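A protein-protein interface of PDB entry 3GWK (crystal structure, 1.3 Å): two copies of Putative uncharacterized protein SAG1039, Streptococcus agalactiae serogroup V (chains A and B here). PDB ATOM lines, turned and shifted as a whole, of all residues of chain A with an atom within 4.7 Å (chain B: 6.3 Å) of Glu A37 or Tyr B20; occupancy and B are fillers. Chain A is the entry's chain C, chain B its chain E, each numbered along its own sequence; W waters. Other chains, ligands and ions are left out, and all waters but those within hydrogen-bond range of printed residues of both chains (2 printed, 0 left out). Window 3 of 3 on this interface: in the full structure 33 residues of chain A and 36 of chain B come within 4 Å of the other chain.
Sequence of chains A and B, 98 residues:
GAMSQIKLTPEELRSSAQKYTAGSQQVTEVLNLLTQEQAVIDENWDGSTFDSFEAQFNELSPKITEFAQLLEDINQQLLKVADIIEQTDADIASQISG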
ATOM      1  N   LEU A  33     -24.015  31.121  23.715  1.00  0.00           N
ATOM      2  CA  LEU A  33     -23.186  31.445  24.837  1.00  0.00           C
ATOM      3  C   LEU A  33     -21.733  31.713  24.437  1.00  0.00           C
ATOM      4  O   LEU A  33     -21.094  32.686  24.886  1.00  0.00           O
ATOM      5  CB  LEU A  33     -23.204  30.303  25.873  1.00  0.00           C
ATOM      6  CG  LEU A  33     -22.368  30.563  27.080  1.00  0.00           C
ATOM      7  CD1 LEU A  33     -23.093  31.621  27.948  1.00  0.00           C
ATOM      8  CD2 LEU A  33     -22.123  29.279  27.821  1.00  0.00           C
ATOM      9  N   LEU A  34     -21.197  30.810  23.640  1.00  0.00           N
ATOM     10  CA  LEU A  34     -19.785  30.900  23.258  1.00  0.00           C
ATOM     11  C   LEU A  34     -19.517  31.959  22.168  1.00  0.00           C
ATOM     12  O   LEU A  34     -18.402  32.462  22.094  1.00  0.00           O
ATOM     13  CB  LEU A  34     -19.268  29.537  22.845  1.00  0.00           C
ATOM     14  CG  LEU A  34     -19.305  28.504  24.029  1.00  0.00           C
ATOM     15  CD1 LEU A  34     -18.757  27.200  23.604  1.00  0.00           C
ATOM     16  CD2 LEU A  34     -18.500  29.064  25.242  1.00  0.00           C
ATOM     17  N   THR A  35     -20.537  32.291  21.380  1.00  0.00           N
ATOM     18  CA  THR A  35     -20.426  33.459  20.535  1.00  0.00           C
ATOM     19  C   THR A  35     -20.214  34.699  21.372  1.00  0.00           C
ATOM     20  O   THR A  35     -19.380  35.581  21.009  1.00  0.00           O
ATOM     21  CB  THR A  35     -21.666  33.587  19.620  1.00  0.00           C
ATOM     22  OG1 THR A  35     -21.652  32.480  18.765  1.00  0.00           O
ATOM     23  CG2 THR A  35     -21.571  34.873  18.741  1.00  0.00           C
ATOM     24  N   GLN A  36     -20.931  34.801  22.500  1.00  0.00           N
ATOM     25  CA  GLN A  36     -20.692  35.961  23.377  1.00  0.00           C
ATOM     26  C   GLN A  36     -19.288  35.886  23.941  1.00  0.00           C
ATOM     27  O   GLN A  36     -18.630  36.892  24.008  1.00  0.00           O
ATOM     28  CB  GLN A  36     -21.718  36.058  24.550  1.00  0.00           C
ATOM     29  CG  GLN A  36     -23.131  36.221  24.140  1.00  0.00           C
ATOM     30  CD  GLN A  36     -24.042  36.252  25.378  1.00  0.00           C
ATOM     31  OE1 GLN A  36     -23.574  36.238  26.553  1.00  0.00           O
ATOM     32  NE2 GLN A  36     -25.347  36.345  25.121  1.00  0.00           N
ATOM     33  N   GLU A  37     -18.889  34.700  24.409  1.00  0.00           N
ATOM     34  CA  GLU A  37     -17.502  34.605  24.982  1.00  0.00           C
ATOM     35  C   GLU A  37     -16.439  34.972  23.944  1.00  0.00           C
ATOM     36  O   GLU A  37     -15.444  35.652  24.254  1.00  0.00           O
ATOM     37  CB  GLU A  37     -17.228  33.171  25.504  1.00  0.00           C
ATOM     38  CG  GLU A  37     -18.079  32.813  26.743  1.00  0.00           C
ATOM     39  CD  GLU A  37     -17.844  33.813  27.883  1.00  0.00           C
ATOM     40  OE1 GLU A  37     -16.715  33.926  28.404  1.00  0.00           O
ATOM     41  OE2 GLU A  37     -18.831  34.453  28.267  1.00  0.00           O
ATOM     42  N   GLN A  38     -16.643  34.578  22.706  1.00  0.00           N
ATOM     43  CA  GLN A  38     -15.690  34.925  21.663  1.00  0.00           C
ATOM     44  C   GLN A  38     -15.541  36.458  21.556  1.00  0.00           C
ATOM     45  O   GLN A  38     -14.431  36.965  21.371  1.00  0.00           O
ATOM     46  CB  GLN A  38     -16.126  34.367  20.287  1.00  0.00           C
ATOM     47  CG  GLN A  38     -15.904  32.843  20.126  1.00  0.00           C
ATOM     48  CD  GLN A  38     -14.433  32.501  19.974  1.00  0.00           C
ATOM     49  OE1 GLN A  38     -13.832  32.579  18.858  1.00  0.00           O
ATOM     50  NE2 GLN A  38     -13.874  32.036  21.025  1.00  0.00           N
ATOM     51  N   ALA A  39     -16.685  37.170  21.624  1.00  0.00           N
ATOM     52  CA  ALA A  39     -16.673  38.628  21.498  1.00  0.00           C
ATOM     53  C   ALA A  39     -16.002  39.270  22.704  1.00  0.00           C
ATOM     54  O   ALA A  39     -15.195  40.214  22.557  1.00  0.00           O
ATOM     55  CB  ALA A  39     -18.136  39.110  21.324  1.00  0.00           C
ATOM     56  N   VAL A  40     -16.262  38.738  23.912  1.00  0.00           N
ATOM     57  CA  VAL A  40     -15.583  39.236  25.089  1.00  0.00           C
ATOM     58  C   VAL A  40     -14.060  39.070  24.977  1.00  0.00           C
ATOM     59  O   VAL A  40     -13.299  39.994  25.296  1.00  0.00           O
ATOM     60  CB  VAL A  40     -16.097  38.613  26.402  1.00  0.00           C
ATOM     61  CG1 VAL A  40     -15.284  39.109  27.589  1.00  0.00           C
ATOM     62  CG2 VAL A  40     -17.596  38.875  26.586  1.00  0.00           C
ATOM     63  N   ILE A  41     -13.625  37.921  24.513  1.00  0.00           N
ATOM     64  CA  ILE A  41     -12.201  37.684  24.359  1.00  0.00           C
ATOM     65  C   ILE A  41     -11.608  38.613  23.327  1.00  0.00           C
ATOM     66  O   ILE A  41     -10.528  39.197  23.505  1.00  0.00           O
ATOM     67  CB  ILE A  41     -11.935  36.220  24.020  1.00  0.00           C
ATOM     68  CG1 ILE A  41     -12.153  35.352  25.296  1.00  0.00           C
ATOM     69  CG2 ILE A  41     -10.480  35.974  23.482  1.00  0.00           C
ATOM     70  CD1 ILE A  41     -12.396  33.891  25.066  1.00  0.00           C
ATOM     71  N   GLU B  12     -10.956  35.664  35.288  1.00  0.00           N
ATOM     72  CA  GLU B  12     -11.930  35.851  34.229  1.00  0.00           C
ATOM     73  C   GLU B  12     -11.675  34.938  33.053  1.00  0.00           C
ATOM     74  O   GLU B  12     -12.598  34.342  32.442  1.00  0.00           O
ATOM     75  CB  GLU B  12     -12.022  37.301  33.776  1.00  0.00           C
ATOM     76  CG  GLU B  12     -12.608  38.254  34.838  1.00  0.00           C
ATOM     77  CD  GLU B  12     -12.463  39.708  34.495  1.00  0.00           C
ATOM     78  OE1 GLU B  12     -11.461  40.060  33.893  1.00  0.00           O
ATOM     79  OE2 GLU B  12     -13.397  40.488  34.870  1.00  0.00           O
ATOM     80  N   SER B  15     -12.901  31.482  34.078  1.00  0.00           N
ATOM     81  CA  SER B  15     -14.379  31.372  34.080  1.00  0.00           C
ATOM     82  C   SER B  15     -14.850  31.198  32.626  1.00  0.00           C
ATOM     83  O   SER B  15     -15.747  30.422  32.320  1.00  0.00           O
ATOM     84  CB  SER B  15     -15.028  32.634  34.682  1.00  0.00           C
ATOM     85  OG  SER B  15     -16.444  32.501  34.748  1.00  0.00           O
ATOM     86  N   SER B  16     -14.209  31.906  31.686  1.00  0.00           N
ATOM     87  CA  SER B  16     -14.596  31.746  30.295  1.00  0.00           C
ATOM     88  C   SER B  16     -14.203  30.332  29.779  1.00  0.00           C
ATOM     89  O   SER B  16     -14.990  29.643  29.134  1.00  0.00           O
ATOM     90  CB  SER B  16     -13.888  32.830  29.468  1.00  0.00           C
ATOM     91  OG  SER B  16     -14.288  32.730  28.111  1.00  0.00           O
ATOM     92  N   ALA B  17     -13.006  29.883  30.139  1.00  0.00           N
ATOM     93  CA  ALA B  17     -12.561  28.550  29.743  1.00  0.00           C
ATOM     94  C   ALA B  17     -13.511  27.445  30.156  1.00  0.00           C
ATOM     95  O   ALA B  17     -13.804  26.551  29.379  1.00  0.00           O
ATOM     96  CB  ALA B  17     -11.171  28.295  30.335  1.00  0.00           C
ATOM     97  N   GLN B  18     -14.055  27.595  31.339  1.00  0.00           N
ATOM     98  CA  GLN B  18     -15.005  26.602  31.849  1.00  0.00           C
ATOM     99  C   GLN B  18     -16.200  26.481  30.913  1.00  0.00           C
ATOM    100  O   GLN B  18     -16.764  25.368  30.689  1.00  0.00           O
ATOM    101  CB  GLN B  18     -15.503  27.099  33.166  1.00  0.00           C
ATOM    102  CG  GLN B  18     -14.713  26.988  34.425  1.00  0.00           C
ATOM    103  CD  GLN B  18     -15.627  27.377  35.640  1.00  0.00           C
ATOM    104  OE1 GLN B  18     -15.517  28.465  36.196  1.00  0.00           O
ATOM    105  NE2 GLN B  18     -16.604  26.506  35.951  1.00  0.00           N
ATOM    106  N   LYS B  19     -16.645  27.605  30.341  1.00  0.00           N
ATOM    107  CA  LYS B  19     -17.796  27.591  29.445  1.00  0.00           C
ATOM    108  C   LYS B  19     -17.492  26.859  28.145  1.00  0.00           C
ATOM    109  O   LYS B  19     -18.310  26.173  27.567  1.00  0.00           O
ATOM    110  CB  LYS B  19     -18.269  29.049  29.164  1.00  0.00           C
ATOM    111  CG  LYS B  19     -18.707  29.777  30.441  1.00  0.00           C
ATOM    112  CD  LYS B  19     -19.079  31.267  30.191  1.00  0.00           C
ATOM    113  CE  LYS B  19     -19.384  31.881  31.643  1.00  0.00           C
ATOM    114  NZ  LYS B  19     -19.593  33.284  31.610  1.00  0.00           N
ATOM    115  N   TYR B  20     -16.245  27.044  27.674  1.00  0.00           N
ATOM    116  CA  TYR B  20     -15.820  26.347  26.457  1.00  0.00           C
ATOM    117  C   TYR B  20     -15.797  24.838  26.622  1.00  0.00           C
ATOM    118  O   TYR B  20     -16.303  24.084  25.784  1.00  0.00           O
ATOM    119  CB  TYR B  20     -14.460  26.843  25.928  1.00  0.00           C
ATOM    120  CG  TYR B  20     -14.583  28.213  25.259  1.00  0.00           C
ATOM    121  CD1 TYR B  20     -14.807  28.318  23.891  1.00  0.00           C
ATOM    122  CD2 TYR B  20     -14.457  29.377  26.015  1.00  0.00           C
ATOM    123  CE1 TYR B  20     -14.933  29.589  23.336  1.00  0.00           C
ATOM    124  CE2 TYR B  20     -14.560  30.629  25.421  1.00  0.00           C
ATOM    125  CZ  TYR B  20     -14.782  30.716  24.070  1.00  0.00           C
ATOM    126  OH  TYR B  20     -14.872  31.967  23.481  1.00  0.00           O
ATOM    127  N   THR B  21     -15.198  24.395  27.716  1.00  0.00           N
ATOM    128  CA  THR B  21     -15.119  22.958  27.898  1.00  0.00           C
ATOM    129  C   THR B  21     -16.491  22.331  28.232  1.00  0.00           C
ATOM    130  O   THR B  21     -16.844  21.242  27.738  1.00  0.00           O
ATOM    131  CB  THR B  21     -14.006  22.581  28.924  1.00  0.00           C
ATOM    132  OG1 THR B  21     -13.847  21.170  28.881  1.00  0.00           O
ATOM    133  CG2 THR B  21     -14.339  23.061  30.283  1.00  0.00           C
ATOM    134  N   ALA B  22     -17.337  23.013  28.971  1.00  0.00           N
ATOM    135  CA  ALA B  22     -18.695  22.554  29.214  1.00  0.00           C
ATOM    136  C   ALA B  22     -19.500  22.491  27.908  1.00  0.00           C
ATOM    137  O   ALA B  22     -20.204  21.533  27.632  1.00  0.00           O
ATOM    138  CB  ALA B  22     -19.383  23.470  30.204  1.00  0.00           C
ATOM    139  N   GLY B  23     -19.314  23.518  27.057  1.00  0.00           N
ATOM    140  CA  GLY B  23     -19.994  23.516  25.784  1.00  0.00           C
ATOM    141  C   GLY B  23     -19.542  22.402  24.892  1.00  0.00           C
ATOM    142  O   GLY B  23     -20.342  21.778  24.163  1.00  0.00           O
ATOM    143  N   SER B  24     -18.245  22.108  24.894  1.00  0.00           N
ATOM    144  CA  SER B  24     -17.702  21.031  24.165  1.00  0.00           C
ATOM    145  C   SER B  24     -18.346  19.704  24.536  1.00  0.00           C
ATOM    146  O   SER B  24     -18.764  18.916  23.685  1.00  0.00           O
ATOM    147  CB  SER B  24     -16.182  20.959  24.382  1.00  0.00           C
ATOM    148  OG  SER B  24     -15.622  19.855  23.685  1.00  0.00           O
ATOM    149  N   GLN B  25     -18.427  19.475  25.835  1.00  0.00           N
ATOM    150  CA  GLN B  25     -19.051  18.227  26.321  1.00  0.00           C
ATOM    151  C   GLN B  25     -20.506  18.126  25.895  1.00  0.00           C
ATOM    152  O   GLN B  25     -20.985  17.041  25.481  1.00  0.00           O
ATOM    153  CB  GLN B  25     -18.927  18.193  27.837  1.00  0.00           C
ATOM    154  CG  GLN B  25     -19.524  16.859  28.374  1.00  0.00           C
ATOM    155  CD  GLN B  25     -19.468  16.745  29.835  1.00  0.00           C
ATOM    156  OE1 GLN B  25     -18.602  17.392  30.508  1.00  0.00           O
ATOM    157  NE2 GLN B  25     -20.389  15.895  30.384  1.00  0.00           N
ATOM    158  N   ALA B  68     -16.496  20.760  18.546  1.00  0.00           N
ATOM    159  CA  ALA B  68     -16.300  20.378  19.928  1.00  0.00           C
ATOM    160  C   ALA B  68     -14.785  20.353  20.236  1.00  0.00           C
ATOM    161  O   ALA B  68     -14.391  20.728  21.372  1.00  0.00           O
ATOM    162  CB  ALA B  68     -16.893  19.007  20.158  1.00  0.00           C
ATOM    163  N   LEU B  70     -12.410  22.213  18.793  1.00  0.00           N
ATOM    164  CA  LEU B  70     -11.999  23.622  18.841  1.00  0.00           C
ATOM    165  C   LEU B  70     -12.292  24.206  20.209  1.00  0.00           C
ATOM    166  O   LEU B  70     -11.493  24.911  20.791  1.00  0.00           O
ATOM    167  CB  LEU B  70     -12.682  24.436  17.712  1.00  0.00           C
ATOM    168  CG  LEU B  70     -12.540  25.948  17.836  1.00  0.00           C
ATOM    169  CD1 LEU B  70     -11.073  26.322  17.544  1.00  0.00           C
ATOM    170  CD2 LEU B  70     -13.447  26.599  16.849  1.00  0.00           C
ATOM    171  N   LEU B  71     -13.482  23.924  20.727  1.00  0.00           N
ATOM    172  CA  LEU B  71     -13.883  24.469  22.018  1.00  0.00           C
ATOM    173  C   LEU B  71     -12.930  23.960  23.127  1.00  0.00           C
ATOM    174  O   LEU B  71     -12.506  24.731  24.032  1.00  0.00           O
ATOM    175  CB  LEU B  71     -15.310  24.104  22.346  1.00  0.00           C
ATOM    176  CG  LEU B  71     -16.379  24.667  21.427  1.00  0.00           C
ATOM    177  CD1 LEU B  71     -17.749  24.251  21.927  1.00  0.00           C
ATOM    178  CD2 LEU B  71     -16.247  26.067  20.934  1.00  0.00           C
ATOM    179  N   GLU B  72     -12.573  22.681  23.067  1.00  0.00           N
ATOM    180  CA  GLU B  72     -11.621  22.153  24.023  1.00  0.00           C
ATOM    181  C   GLU B  72     -10.245  22.810  23.861  1.00  0.00           C
ATOM    182  O   GLU B  72      -9.546  23.128  24.858  1.00  0.00           O
ATOM    183  CB  GLU B  72     -11.561  20.636  23.901  1.00  0.00           C
ATOM    184  CG  GLU B  72     -10.750  20.001  25.065  1.00  0.00           C
ATOM    185  CD  GLU B  72     -11.128  20.416  26.506  1.00  0.00           C
ATOM    186  OE1 GLU B  72     -12.365  20.456  26.742  1.00  0.00           O
ATOM    187  OE2 GLU B  72     -10.203  20.649  27.344  1.00  0.00           O
ATOM    188  N   ILE B  74      -9.610  25.872  22.780  1.00  0.00           N
ATOM    189  CA  ILE B  74      -9.710  27.209  23.309  1.00  0.00           C
ATOM    190  C   ILE B  74      -9.623  27.145  24.829  1.00  0.00           C
ATOM    191  O   ILE B  74      -8.885  27.922  25.424  1.00  0.00           O
ATOM    192  CB  ILE B  74     -11.008  27.914  22.840  1.00  0.00           C
ATOM    193  CG1 ILE B  74     -10.947  28.156  21.324  1.00  0.00           C
ATOM    194  CG2 ILE B  74     -11.249  29.193  23.609  1.00  0.00           C
ATOM    195  CD1 ILE B  74     -12.314  28.535  20.722  1.00  0.00           C
ATOM    196  N   ASN B  75     -10.357  26.244  25.462  1.00  0.00           N
ATOM    197  CA  ASN B  75     -10.264  26.032  26.900  1.00  0.00           C
ATOM    198  C   ASN B  75      -8.793  25.887  27.310  1.00  0.00           C
ATOM    199  O   ASN B  75      -8.258  26.525  28.214  1.00  0.00           O
ATOM    200  CB  ASN B  75     -11.050  24.786  27.311  1.00  0.00           C
ATOM    201  CG  ASN B  75     -10.765  24.366  28.735  1.00  0.00           C
ATOM    202  OD1 ASN B  75     -10.981  25.096  29.685  1.00  0.00           O
ATOM    203  ND2 ASN B  75     -10.266  23.209  28.898  1.00  0.00           N
ATOM    204  N   LEU B  78      -6.713  29.071  26.900  1.00  0.00           N
ATOM    205  CA  LEU B  78      -7.126  30.075  27.908  1.00  0.00           C
ATOM    206  C   LEU B  78      -6.520  29.747  29.287  1.00  0.00           C
ATOM    207  O   LEU B  78      -6.059  30.650  29.975  1.00  0.00           O
ATOM    208  CB  LEU B  78      -8.638  30.170  28.015  1.00  0.00           C
ATOM    209  CG  LEU B  78      -9.360  30.898  26.877  1.00  0.00           C
ATOM    210  CD1 LEU B  78     -10.896  30.610  27.040  1.00  0.00           C
ATOM    211  CD2 LEU B  78      -9.070  32.392  26.946  1.00  0.00           C
HETATM  212  O   HOH W   1     -14.814  35.763  27.671  1.00  0.00           O
HETATM  213  O   HOH W   2     -17.063  33.986  31.138  1.00  0.00           O
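No position is printed for both chains.
Water W2 lies within hydrogen-bond range of the side-chain amino group (NZ) of Lys B19 and the side-chain carboxylate (OE1) of Glu A37.
Water W1 lies within hydrogen-bond range of OE1 of Glu A37 and OG of Ser B16.
Of the 19 printed residues of chain B, 5 touch a printed residue of chain A.
Of the 9 printed residues of chain A, 4 touch a printed residue of chain B.
Along chain A the printed residues that touch a printed residue of chain B span positions 34 to 41.
Among the printed residues, 10 pairs touch across the chains.
Among the printed residues, Asp or Glu carboxylates within 4 Å of a Lys or Arg side-chain nitrogen of the other chain: Glu A37 with Lys B19.
Printed residues of chain B within 4 Å of Leu A34: Lys B19 (3.7 Å), Tyr B20 (3.8 Å) and Leu B71 (3.5 Å).
Glu A37 touches three residues of chain B.
Of the printed residues of chain B, Ile A41 touches Ser B16 (3.8 Å) and Tyr B20 (3.5 Å).
Of the printed residues of chain A, Ser B16 touches Glu A37 and Ile A41.
Asn B75 touches none of the printed residues of chain A.
The nearest printed residue of chain B that does not touch Glu A37 is Ser B15 (5.3 Å).
The nearest printed residue of chain A that does not touch Tyr B20 is Ala A39 (5.8 Å).
The nearest printed residue of chain A that does not touch Ser B16 is Leu A34 (5.3 Å).
Among the printed residues, pairs that only touch across the chains: Leu A34 with Lys B19 (3.7 Å), Leu A34 with Tyr B20 (3.8 Å), Leu A34 with Leu B71 (3.5 Å), Glu A37 with Tyr B20 (3.3 Å), Gln A38 with Ile B74 (3.8 Å), Ile A41 with Ser B16 (3.8 Å) and Ile A41 with Tyr B20 (3.5 Å).
The side-chain hydroxyl (OG) of Ser B16 lies within hydrogen-bond range of the side-chain carboxylate (OE1) of Glu A37, at 2.7 Å.
NE2 of Gln A38 lies within hydrogen-bond range of OH of Tyr B20 (2.7 Å).
NZ of Lys B19 is in salt-bridge range of OE2 of Glu A37 (3.6 Å).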
